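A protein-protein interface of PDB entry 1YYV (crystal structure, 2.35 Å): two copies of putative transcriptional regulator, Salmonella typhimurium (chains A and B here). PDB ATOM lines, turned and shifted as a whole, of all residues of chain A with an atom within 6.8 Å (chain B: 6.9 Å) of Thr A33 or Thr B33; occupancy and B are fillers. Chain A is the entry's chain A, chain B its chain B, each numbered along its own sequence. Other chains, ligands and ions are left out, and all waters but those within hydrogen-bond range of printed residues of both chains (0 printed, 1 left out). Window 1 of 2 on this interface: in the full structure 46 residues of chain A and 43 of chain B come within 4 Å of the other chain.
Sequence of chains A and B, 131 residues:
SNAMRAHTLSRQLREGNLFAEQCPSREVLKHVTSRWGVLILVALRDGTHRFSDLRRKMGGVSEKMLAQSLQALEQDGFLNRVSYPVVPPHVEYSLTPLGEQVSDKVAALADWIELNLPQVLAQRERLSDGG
Ile B113 touches Val A28 (CG2 to CG1, 3.96 Å).
Ile B113 touches Leu A29 (CD1 to CA, 3.9 Å).
Val A32 touches Ile B113.
Thr A33 touches Thr B33 (CG2 to OG1, 3.4 Å).
CD2 of Leu B29 touches CG2 of Val A38, at 3.9 Å.
OG1 of Thr B33 touches CD2 of Leu A109 (3.7 Å).
Leu A109 touches Val B106 (CD1 to CG2, 3.6 Å).
CG2 of Ile A113 touches CG2 of Val B28, 2.8 Å away.
CD1 of Ile A113 touches CA of Leu B29, 3.8 Å away.
Ile A113 touches Val B32.
Thr A33 touches just these residues of chain B: Thr B33 and Leu B109.
Printed residues of chain A within 4 Å of Val B28: Ile A113 (2.8 Å).
Of chain A, only Thr A33 and Leu A109 come within 4 Å of Thr B33.
Of the printed residues of chain A, Val B106 touches Leu A109.
The nearest residue of chain B that does not touch Thr A33 is Leu B29 (4.4 Å).
The nearest residue of chain A that does not touch Thr B33 is Leu A29 (4.3 Å).
Of the 16 printed residues of chain A, 7 touch a printed residue of chain B.
Along chain A the printed residues that touch a printed residue of chain B span positions 28 to 113.
Printed residues of chain B that touch a printed residue of chain A: Val B28, Leu B29, Val B32, Thr B33, Val B106, Leu B109 and Ile B113.
Hydrophobic or aromatic side chains of chain B within 4 Å of the printed part of chain A: Val B28, Leu B29, Val B32, Val B106, Leu B109 and Ile B113.
Among the printed residues, no Asp or Glu carboxylate lies within 4 Å of a Lys or Arg side-chain nitrogen of the other chain.
Thr A33 touches its own counterpart, Thr B33.
Thr A33 touches Leu B109, and with the chains exchanged Leu A109 touches Thr B33.
Val A38 touches Leu B29, but with the chains exchanged Leu A29 does not touch Val B38 (4.2 Å).
Leu A109 touches Val B106, but with the chains exchanged Val A106 does not touch Leu B109 (4.02 Å).
Positions printed for both chains: 28, 29, 30, 31, 32, 33, 34, 35, 36, 37, 38, 41, 73, 106, 109 and 113.
The backbone carbonyl oxygen of Leu A29 lies within hydrogen-bond range of the side-chain hydroxyl of Thr A33.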
ATOM      1  N   VAL A  28       0.951 -18.912   3.422  1.00  0.00           N
ATOM      2  CA  VAL A  28       0.473 -20.213   2.936  1.00  0.00           C
ATOM      3  C   VAL A  28      -0.543 -20.041   1.820  1.00  0.00           C
ATOM      4  O   VAL A  28      -0.462 -20.700   0.815  1.00  0.00           O
ATOM      5  CB  VAL A  28      -0.135 -21.043   4.070  1.00  0.00           C
ATOM      6  CG1 VAL A  28      -0.666 -22.419   3.541  1.00  0.00           C
ATOM      7  CG2 VAL A  28       0.874 -21.140   5.259  1.00  0.00           C
ATOM      8  N   LEU A  29      -1.483 -19.133   1.979  1.00  0.00           N
ATOM      9  CA  LEU A  29      -2.473 -18.881   0.926  1.00  0.00           C
ATOM     10  C   LEU A  29      -1.825 -18.418  -0.392  1.00  0.00           C
ATOM     11  O   LEU A  29      -2.155 -18.925  -1.428  1.00  0.00           O
ATOM     12  CB  LEU A  29      -3.544 -17.912   1.419  1.00  0.00           C
ATOM     13  CG  LEU A  29      -4.426 -17.329   0.330  1.00  0.00           C
ATOM     14  CD1 LEU A  29      -5.521 -18.314  -0.035  1.00  0.00           C
ATOM     15  CD2 LEU A  29      -4.977 -15.957   0.739  1.00  0.00           C
ATOM     16  N   LYS A  30      -0.888 -17.476  -0.311  1.00  0.00           N
ATOM     17  CA  LYS A  30      -0.084 -17.057  -1.440  1.00  0.00           C
ATOM     18  C   LYS A  30       0.670 -18.247  -2.111  1.00  0.00           C
ATOM     19  O   LYS A  30       0.622 -18.436  -3.347  1.00  0.00           O
ATOM     20  CB  LYS A  30       0.922 -15.970  -0.999  1.00  0.00           C
ATOM     21  CG  LYS A  30       1.715 -15.423  -2.191  1.00  0.00           C
ATOM     22  CD  LYS A  30       2.826 -14.380  -1.872  1.00  0.00           C
ATOM     23  CE  LYS A  30       2.452 -12.986  -2.443  1.00  0.00           C
ATOM     24  NZ  LYS A  30       3.593 -12.046  -2.922  1.00  0.00           N
ATOM     25  N   HIS A  31       1.370 -19.047  -1.317  1.00  0.00           N
ATOM     26  CA  HIS A  31       2.094 -20.179  -1.915  1.00  0.00           C
ATOM     27  C   HIS A  31       1.195 -21.135  -2.682  1.00  0.00           C
ATOM     28  O   HIS A  31       1.581 -21.602  -3.750  1.00  0.00           O
ATOM     29  CB  HIS A  31       2.930 -20.942  -0.879  1.00  0.00           C
ATOM     30  CG  HIS A  31       3.928 -20.067  -0.175  1.00  0.00           C
ATOM     31  ND1 HIS A  31       4.468 -20.378   1.064  1.00  0.00           N
ATOM     32  CD2 HIS A  31       4.476 -18.881  -0.540  1.00  0.00           C
ATOM     33  CE1 HIS A  31       5.320 -19.430   1.413  1.00  0.00           C
ATOM     34  NE2 HIS A  31       5.324 -18.502   0.472  1.00  0.00           N
ATOM     35  N   VAL A  32       0.001 -21.422  -2.159  1.00  0.00           N
ATOM     36  CA  VAL A  32      -0.801 -22.521  -2.746  1.00  0.00           C
ATOM     37  C   VAL A  32      -1.697 -22.021  -3.871  1.00  0.00           C
ATOM     38  O   VAL A  32      -2.320 -22.800  -4.609  1.00  0.00           O
ATOM     39  CB  VAL A  32      -1.564 -23.404  -1.659  1.00  0.00           C
ATOM     40  CG1 VAL A  32      -0.625 -23.813  -0.532  1.00  0.00           C
ATOM     41  CG2 VAL A  32      -2.824 -22.699  -1.087  1.00  0.00           C
ATOM     42  N   THR A  33      -1.788 -20.705  -4.003  1.00  0.00           N
ATOM     43  CA  THR A  33      -2.653 -20.175  -5.035  1.00  0.00           C
ATOM     44  C   THR A  33      -1.954 -19.248  -6.032  1.00  0.00           C
ATOM     45  O   THR A  33      -2.629 -18.675  -6.906  1.00  0.00           O
ATOM     46  CB  THR A  33      -3.889 -19.493  -4.440  1.00  0.00           C
ATOM     47  OG1 THR A  33      -3.469 -18.475  -3.542  1.00  0.00           O
ATOM     48  CG2 THR A  33      -4.821 -20.503  -3.735  1.00  0.00           C
ATOM     49  N   SER A  34      -0.629 -19.095  -5.877  1.00  0.00           N
ATOM     50  CA  SER A  34       0.193 -18.470  -6.879  1.00  0.00           C
ATOM     51  C   SER A  34      -0.004 -19.279  -8.128  1.00  0.00           C
ATOM     52  O   SER A  34      -0.441 -20.411  -8.084  1.00  0.00           O
ATOM     53  CB  SER A  34       1.684 -18.439  -6.506  1.00  0.00           C
ATOM     54  OG  SER A  34       2.239 -19.747  -6.581  1.00  0.00           O
ATOM     55  N   ARG A  35       0.314 -18.682  -9.253  1.00  0.00           N
ATOM     56  CA  ARG A  35       0.041 -19.311 -10.527  1.00  0.00           C
ATOM     57  C   ARG A  35       0.874 -20.588 -10.744  1.00  0.00           C
ATOM     58  O   ARG A  35       0.413 -21.513 -11.380  1.00  0.00           O
ATOM     59  CB  ARG A  35       0.234 -18.247 -11.599  1.00  0.00           C
ATOM     60  CG  ARG A  35       0.784 -18.635 -12.922  1.00  0.00           C
ATOM     61  CD  ARG A  35       0.855 -17.345 -13.646  1.00  0.00           C
ATOM     62  NE  ARG A  35       1.476 -17.452 -14.948  1.00  0.00           N
ATOM     63  CZ  ARG A  35       1.629 -16.422 -15.764  1.00  0.00           C
ATOM     64  NH1 ARG A  35       1.176 -15.226 -15.383  1.00  0.00           N
ATOM     65  NH2 ARG A  35       2.222 -16.590 -16.950  1.00  0.00           N
ATOM     66  N   TRP A  36       2.078 -20.652 -10.186  1.00  0.00           N
ATOM     67  CA  TRP A  36       2.855 -21.885 -10.260  1.00  0.00           C
ATOM     68  C   TRP A  36       2.519 -22.864  -9.143  1.00  0.00           C
ATOM     69  O   TRP A  36       2.519 -24.070  -9.376  1.00  0.00           O
ATOM     70  CB  TRP A  36       4.359 -21.601 -10.372  1.00  0.00           C
ATOM     71  CG  TRP A  36       4.662 -20.531 -11.437  1.00  0.00           C
ATOM     72  CD1 TRP A  36       5.350 -19.354 -11.253  1.00  0.00           C
ATOM     73  CD2 TRP A  36       4.246 -20.539 -12.822  1.00  0.00           C
ATOM     74  NE1 TRP A  36       5.397 -18.653 -12.427  1.00  0.00           N
ATOM     75  CE2 TRP A  36       4.730 -19.348 -13.407  1.00  0.00           C
ATOM     76  CE3 TRP A  36       3.522 -21.444 -13.625  1.00  0.00           C
ATOM     77  CZ2 TRP A  36       4.511 -19.028 -14.766  1.00  0.00           C
ATOM     78  CZ3 TRP A  36       3.312 -21.133 -14.975  1.00  0.00           C
ATOM     79  CH2 TRP A  36       3.798 -19.929 -15.524  1.00  0.00           C
ATOM     80  N   GLY A  37       2.161 -22.364  -7.954  1.00  0.00           N
ATOM     81  CA  GLY A  37       1.776 -23.261  -6.847  1.00  0.00           C
ATOM     82  C   GLY A  37       0.552 -24.100  -7.150  1.00  0.00           C
ATOM     83  O   GLY A  37       0.508 -25.288  -6.811  1.00  0.00           O
ATOM     84  N   VAL A  38      -0.444 -23.491  -7.792  1.00  0.00           N
ATOM     85  CA  VAL A  38      -1.666 -24.192  -8.165  1.00  0.00           C
ATOM     86  C   VAL A  38      -1.356 -25.341  -9.148  1.00  0.00           C
ATOM     87  O   VAL A  38      -1.898 -26.426  -9.049  1.00  0.00           O
ATOM     88  CB  VAL A  38      -2.715 -23.254  -8.864  1.00  0.00           C
ATOM     89  CG1 VAL A  38      -3.927 -24.073  -9.360  1.00  0.00           C
ATOM     90  CG2 VAL A  38      -3.217 -22.144  -7.940  1.00  0.00           C
ATOM     91  N   LEU A  41       0.476 -28.175  -7.520  1.00  0.00           N
ATOM     92  CA  LEU A  41      -0.420 -28.951  -6.671  1.00  0.00           C
ATOM     93  C   LEU A  41      -1.446 -29.777  -7.432  1.00  0.00           C
ATOM     94  O   LEU A  41      -1.865 -30.841  -6.957  1.00  0.00           O
ATOM     95  CB  LEU A  41      -1.125 -28.043  -5.652  1.00  0.00           C
ATOM     96  CG  LEU A  41      -0.238 -27.526  -4.527  1.00  0.00           C
ATOM     97  CD1 LEU A  41      -1.013 -26.553  -3.687  1.00  0.00           C
ATOM     98  CD2 LEU A  41       0.379 -28.654  -3.619  1.00  0.00           C
ATOM     99  N   LEU A  73       6.566 -24.600  -1.153  1.00  0.00           N
ATOM    100  CA  LEU A  73       5.629 -25.688  -0.899  1.00  0.00           C
ATOM    101  C   LEU A  73       6.225 -26.816  -0.083  1.00  0.00           C
ATOM    102  O   LEU A  73       5.513 -27.436   0.714  1.00  0.00           O
ATOM    103  CB  LEU A  73       5.026 -26.220  -2.209  1.00  0.00           C
ATOM    104  CG  LEU A  73       4.116 -25.271  -3.023  1.00  0.00           C
ATOM    105  CD1 LEU A  73       3.725 -25.857  -4.411  1.00  0.00           C
ATOM    106  CD2 LEU A  73       2.854 -24.912  -2.244  1.00  0.00           C
ATOM    107  N   VAL A 106      -7.462 -26.857  -3.629  1.00  0.00           N
ATOM    108  CA  VAL A 106      -7.012 -26.025  -4.721  1.00  0.00           C
ATOM    109  C   VAL A 106      -7.625 -26.501  -6.020  1.00  0.00           C
ATOM    110  O   VAL A 106      -8.121 -25.678  -6.795  1.00  0.00           O
ATOM    111  CB  VAL A 106      -5.448 -25.916  -4.777  1.00  0.00           C
ATOM    112  CG1 VAL A 106      -5.001 -25.225  -6.049  1.00  0.00           C
ATOM    113  CG2 VAL A 106      -4.946 -25.126  -3.563  1.00  0.00           C
ATOM    114  N   LEU A 109     -11.387 -25.790  -6.551  1.00  0.00           N
ATOM    115  CA  LEU A 109     -11.495 -24.383  -6.998  1.00  0.00           C
ATOM    116  C   LEU A 109     -11.077 -24.167  -8.459  1.00  0.00           C
ATOM    117  O   LEU A 109     -11.794 -23.503  -9.217  1.00  0.00           O
ATOM    118  CB  LEU A 109     -10.712 -23.437  -6.069  1.00  0.00           C
ATOM    119  CG  LEU A 109     -10.661 -21.931  -6.355  1.00  0.00           C
ATOM    120  CD1 LEU A 109     -12.016 -21.275  -6.186  1.00  0.00           C
ATOM    121  CD2 LEU A 109      -9.633 -21.314  -5.443  1.00  0.00           C
ATOM    122  N   ILE A 113     -13.550 -23.210 -11.686  1.00  0.00           N
ATOM    123  CA  ILE A 113     -13.257 -22.061 -12.528  1.00  0.00           C
ATOM    124  C   ILE A 113     -13.176 -22.483 -14.004  1.00  0.00           C
ATOM    125  O   ILE A 113     -13.799 -21.855 -14.839  1.00  0.00           O
ATOM    126  CB  ILE A 113     -11.997 -21.315 -12.066  1.00  0.00           C
ATOM    127  CG1 ILE A 113     -12.239 -20.678 -10.702  1.00  0.00           C
ATOM    128  CG2 ILE A 113     -11.611 -20.250 -13.062  1.00  0.00           C
ATOM    129  CD1 ILE A 113     -11.058 -19.922 -10.154  1.00  0.00           C
ATOM    130  N   VAL B  28      -9.248 -15.065 -13.794  1.00  0.00           N
ATOM    131  CA  VAL B  28     -10.314 -15.248 -12.840  1.00  0.00           C
ATOM    132  C   VAL B  28      -9.769 -15.911 -11.562  1.00  0.00           C
ATOM    133  O   VAL B  28     -10.138 -15.527 -10.479  1.00  0.00           O
ATOM    134  CB  VAL B  28     -11.558 -16.021 -13.425  1.00  0.00           C
ATOM    135  CG1 VAL B  28     -11.900 -15.569 -14.827  1.00  0.00           C
ATOM    136  CG2 VAL B  28     -11.292 -17.456 -13.477  1.00  0.00           C
ATOM    137  N   LEU B  29      -8.866 -16.863 -11.702  1.00  0.00           N
ATOM    138  CA  LEU B  29      -8.196 -17.494 -10.558  1.00  0.00           C
ATOM    139  C   LEU B  29      -7.418 -16.493  -9.718  1.00  0.00           C
ATOM    140  O   LEU B  29      -7.508 -16.514  -8.505  1.00  0.00           O
ATOM    141  CB  LEU B  29      -7.259 -18.611 -11.035  1.00  0.00           C
ATOM    142  CG  LEU B  29      -6.371 -19.223  -9.942  1.00  0.00           C
ATOM    143  CD1 LEU B  29      -7.118 -20.345  -9.209  1.00  0.00           C
ATOM    144  CD2 LEU B  29      -5.006 -19.707 -10.477  1.00  0.00           C
ATOM    145  N   LYS B  30      -6.645 -15.632 -10.378  1.00  0.00           N
ATOM    146  CA  LYS B  30      -5.922 -14.527  -9.742  1.00  0.00           C
ATOM    147  C   LYS B  30      -6.875 -13.641  -8.904  1.00  0.00           C
ATOM    148  O   LYS B  30      -6.560 -13.250  -7.770  1.00  0.00           O
ATOM    149  CB  LYS B  30      -5.254 -13.716 -10.833  1.00  0.00           C
ATOM    150  CG  LYS B  30      -4.150 -12.802 -10.359  1.00  0.00           C
ATOM    151  CD  LYS B  30      -3.625 -11.956 -11.513  1.00  0.00           C
ATOM    152  CE  LYS B  30      -3.387 -10.499 -11.071  1.00  0.00           C
ATOM    153  NZ  LYS B  30      -2.653  -9.652 -12.130  1.00  0.00           N
ATOM    154  N   HIS B  31      -8.063 -13.393  -9.443  1.00  0.00           N
ATOM    155  CA  HIS B  31      -9.042 -12.518  -8.816  1.00  0.00           C
ATOM    156  C   HIS B  31      -9.702 -13.149  -7.613  1.00  0.00           C
ATOM    157  O   HIS B  31     -10.024 -12.432  -6.691  1.00  0.00           O
ATOM    158  CB  HIS B  31     -10.185 -12.138  -9.776  1.00  0.00           C
ATOM    159  CG  HIS B  31      -9.753 -11.350 -10.967  1.00  0.00           C
ATOM    160  ND1 HIS B  31     -10.540 -11.218 -12.093  1.00  0.00           N
ATOM    161  CD2 HIS B  31      -8.624 -10.638 -11.204  1.00  0.00           C
ATOM    162  CE1 HIS B  31      -9.918 -10.452 -12.965  1.00  0.00           C
ATOM    163  NE2 HIS B  31      -8.744 -10.107 -12.462  1.00  0.00           N
ATOM    164  N   VAL B  32      -9.965 -14.461  -7.623  1.00  0.00           N
ATOM    165  CA  VAL B  32     -10.747 -15.022  -6.516  1.00  0.00           C
ATOM    166  C   VAL B  32      -9.827 -15.475  -5.403  1.00  0.00           C
ATOM    167  O   VAL B  32     -10.253 -15.815  -4.319  1.00  0.00           O
ATOM    168  CB  VAL B  32     -11.782 -16.142  -6.962  1.00  0.00           C
ATOM    169  CG1 VAL B  32     -12.608 -15.661  -8.122  1.00  0.00           C
ATOM    170  CG2 VAL B  32     -11.071 -17.463  -7.341  1.00  0.00           C
ATOM    171  N   THR B  33      -8.545 -15.427  -5.678  1.00  0.00           N
ATOM    172  CA  THR B  33      -7.597 -16.116  -4.878  1.00  0.00           C
ATOM    173  C   THR B  33      -6.567 -15.129  -4.334  1.00  0.00           C
ATOM    174  O   THR B  33      -5.736 -15.488  -3.495  1.00  0.00           O
ATOM    175  CB  THR B  33      -7.004 -17.276  -5.767  1.00  0.00           C
ATOM    176  OG1 THR B  33      -7.230 -18.545  -5.129  1.00  0.00           O
ATOM    177  CG2 THR B  33      -5.607 -17.053  -6.199  1.00  0.00           C
ATOM    178  N   SER B  34      -6.649 -13.865  -4.790  1.00  0.00           N
ATOM    179  CA  SER B  34      -5.854 -12.817  -4.189  1.00  0.00           C
ATOM    180  C   SER B  34      -6.276 -12.650  -2.725  1.00  0.00           C
ATOM    181  O   SER B  34      -7.397 -13.023  -2.322  1.00  0.00           O
ATOM    182  CB  SER B  34      -5.967 -11.480  -4.967  1.00  0.00           C
ATOM    183  OG  SER B  34      -7.235 -10.855  -4.754  1.00  0.00           O
ATOM    184  N   ARG B  35      -5.362 -12.104  -1.940  1.00  0.00           N
ATOM    185  CA  ARG B  35      -5.559 -11.916  -0.523  1.00  0.00           C
ATOM    186  C   ARG B  35      -6.852 -11.170  -0.260  1.00  0.00           C
ATOM    187  O   ARG B  35      -7.630 -11.552   0.580  1.00  0.00           O
ATOM    188  CB  ARG B  35      -4.424 -11.053   0.003  1.00  0.00           C
ATOM    189  CG  ARG B  35      -4.542 -10.828   1.478  1.00  0.00           C
ATOM    190  CD  ARG B  35      -3.191 -11.028   2.046  1.00  0.00           C
ATOM    191  NE  ARG B  35      -2.568  -9.788   2.387  1.00  0.00           N
ATOM    192  CZ  ARG B  35      -1.256  -9.623   2.481  1.00  0.00           C
ATOM    193  NH1 ARG B  35      -0.413 -10.627   2.191  1.00  0.00           N
ATOM    194  NH2 ARG B  35      -0.798  -8.430   2.818  1.00  0.00           N
ATOM    195  N   TRP B  36      -7.068 -10.086  -0.991  1.00  0.00           N
ATOM    196  CA  TRP B  36      -8.243  -9.283  -0.807  1.00  0.00           C
ATOM    197  C   TRP B  36      -9.507  -9.954  -1.386  1.00  0.00           C
ATOM    198  O   TRP B  36     -10.555  -9.904  -0.755  1.00  0.00           O
ATOM    199  CB  TRP B  36      -7.975  -7.876  -1.378  1.00  0.00           C
ATOM    200  CG  TRP B  36      -6.712  -7.226  -0.789  1.00  0.00           C
ATOM    201  CD1 TRP B  36      -5.719  -6.542  -1.476  1.00  0.00           C
ATOM    202  CD2 TRP B  36      -6.306  -7.224   0.602  1.00  0.00           C
ATOM    203  NE1 TRP B  36      -4.752  -6.077  -0.579  1.00  0.00           N
ATOM    204  CE2 TRP B  36      -5.093  -6.477   0.691  1.00  0.00           C
ATOM    205  CE3 TRP B  36      -6.853  -7.782   1.781  1.00  0.00           C
ATOM    206  CZ2 TRP B  36      -4.402  -6.312   1.902  1.00  0.00           C
ATOM    207  CZ3 TRP B  36      -6.201  -7.560   2.996  1.00  0.00           C
ATOM    208  CH2 TRP B  36      -4.983  -6.832   3.041  1.00  0.00           C
ATOM    209  N   GLY B  37      -9.374 -10.617  -2.534  1.00  0.00           N
ATOM    210  CA  GLY B  37     -10.468 -11.307  -3.186  1.00  0.00           C
ATOM    211  C   GLY B  37     -11.018 -12.432  -2.291  1.00  0.00           C
ATOM    212  O   GLY B  37     -12.241 -12.635  -2.178  1.00  0.00           O
ATOM    213  N   VAL B  38     -10.108 -13.150  -1.656  1.00  0.00           N
ATOM    214  CA  VAL B  38     -10.493 -14.250  -0.732  1.00  0.00           C
ATOM    215  C   VAL B  38     -11.320 -13.677   0.417  1.00  0.00           C
ATOM    216  O   VAL B  38     -12.344 -14.196   0.760  1.00  0.00           O
ATOM    217  CB  VAL B  38      -9.214 -15.002  -0.200  1.00  0.00           C
ATOM    218  CG1 VAL B  38      -9.524 -15.891   1.074  1.00  0.00           C
ATOM    219  CG2 VAL B  38      -8.626 -15.822  -1.323  1.00  0.00           C
ATOM    220  N   LEU B  41     -14.849 -12.472  -0.658  1.00  0.00           N
ATOM    221  CA  LEU B  41     -15.741 -13.612  -0.905  1.00  0.00           C
ATOM    222  C   LEU B  41     -16.165 -14.350   0.334  1.00  0.00           C
ATOM    223  O   LEU B  41     -17.279 -14.823   0.401  1.00  0.00           O
ATOM    224  CB  LEU B  41     -15.147 -14.590  -1.942  1.00  0.00           C
ATOM    225  CG  LEU B  41     -15.011 -14.016  -3.364  1.00  0.00           C
ATOM    226  CD1 LEU B  41     -14.191 -14.957  -4.247  1.00  0.00           C
ATOM    227  CD2 LEU B  41     -16.374 -13.709  -4.007  1.00  0.00           C
ATOM    228  N   LEU B  73     -14.114  -8.653  -9.083  1.00  0.00           N
ATOM    229  CA  LEU B  73     -15.148  -9.639  -8.735  1.00  0.00           C
ATOM    230  C   LEU B  73     -16.549  -9.305  -9.269  1.00  0.00           C
ATOM    231  O   LEU B  73     -17.302 -10.208  -9.613  1.00  0.00           O
ATOM    232  CB  LEU B  73     -15.190  -9.881  -7.236  1.00  0.00           C
ATOM    233  CG  LEU B  73     -13.863 -10.328  -6.591  1.00  0.00           C
ATOM    234  CD1 LEU B  73     -14.046 -10.339  -5.072  1.00  0.00           C
ATOM    235  CD2 LEU B  73     -13.435 -11.723  -7.113  1.00  0.00           C
ATOM    236  N   VAL B 106     -13.814 -21.087  -2.352  1.00  0.00           N
ATOM    237  CA  VAL B 106     -12.814 -20.234  -1.798  1.00  0.00           C
ATOM    238  C   VAL B 106     -12.750 -20.348  -0.295  1.00  0.00           C
ATOM    239  O   VAL B 106     -11.634 -20.487   0.242  1.00  0.00           O
ATOM    240  CB  VAL B 106     -12.897 -18.740  -2.298  1.00  0.00           C
ATOM    241  CG1 VAL B 106     -12.058 -17.851  -1.366  1.00  0.00           C
ATOM    242  CG2 VAL B 106     -12.439 -18.624  -3.770  1.00  0.00           C
ATOM    243  N   LEU B 109     -11.186 -23.487   1.154  1.00  0.00           N
ATOM    244  CA  LEU B 109      -9.731 -23.395   1.068  1.00  0.00           C
ATOM    245  C   LEU B 109      -9.164 -22.480   2.176  1.00  0.00           C
ATOM    246  O   LEU B 109      -8.179 -22.834   2.846  1.00  0.00           O
ATOM    247  CB  LEU B 109      -9.281 -22.939  -0.350  1.00  0.00           C
ATOM    248  CG  LEU B 109      -7.768 -22.613  -0.499  1.00  0.00           C
ATOM    249  CD1 LEU B 109      -6.853 -23.841  -0.268  1.00  0.00           C
ATOM    250  CD2 LEU B 109      -7.441 -22.049  -1.871  1.00  0.00           C
ATOM    251  N   ILE B 113      -6.729 -23.842   5.301  1.00  0.00           N
ATOM    252  CA  ILE B 113      -5.457 -23.181   5.583  1.00  0.00           C
ATOM    253  C   ILE B 113      -5.393 -22.677   7.011  1.00  0.00           C
ATOM    254  O   ILE B 113      -4.429 -22.933   7.684  1.00  0.00           O
ATOM    255  CB  ILE B 113      -5.151 -22.014   4.572  1.00  0.00           C
ATOM    256  CG1 ILE B 113      -4.741 -22.605   3.195  1.00  0.00           C
ATOM    257  CG2 ILE B 113      -4.038 -21.097   5.135  1.00  0.00           C
ATOM    258  CD1 ILE B 113      -4.934 -21.690   2.065  1.00  0.00           C
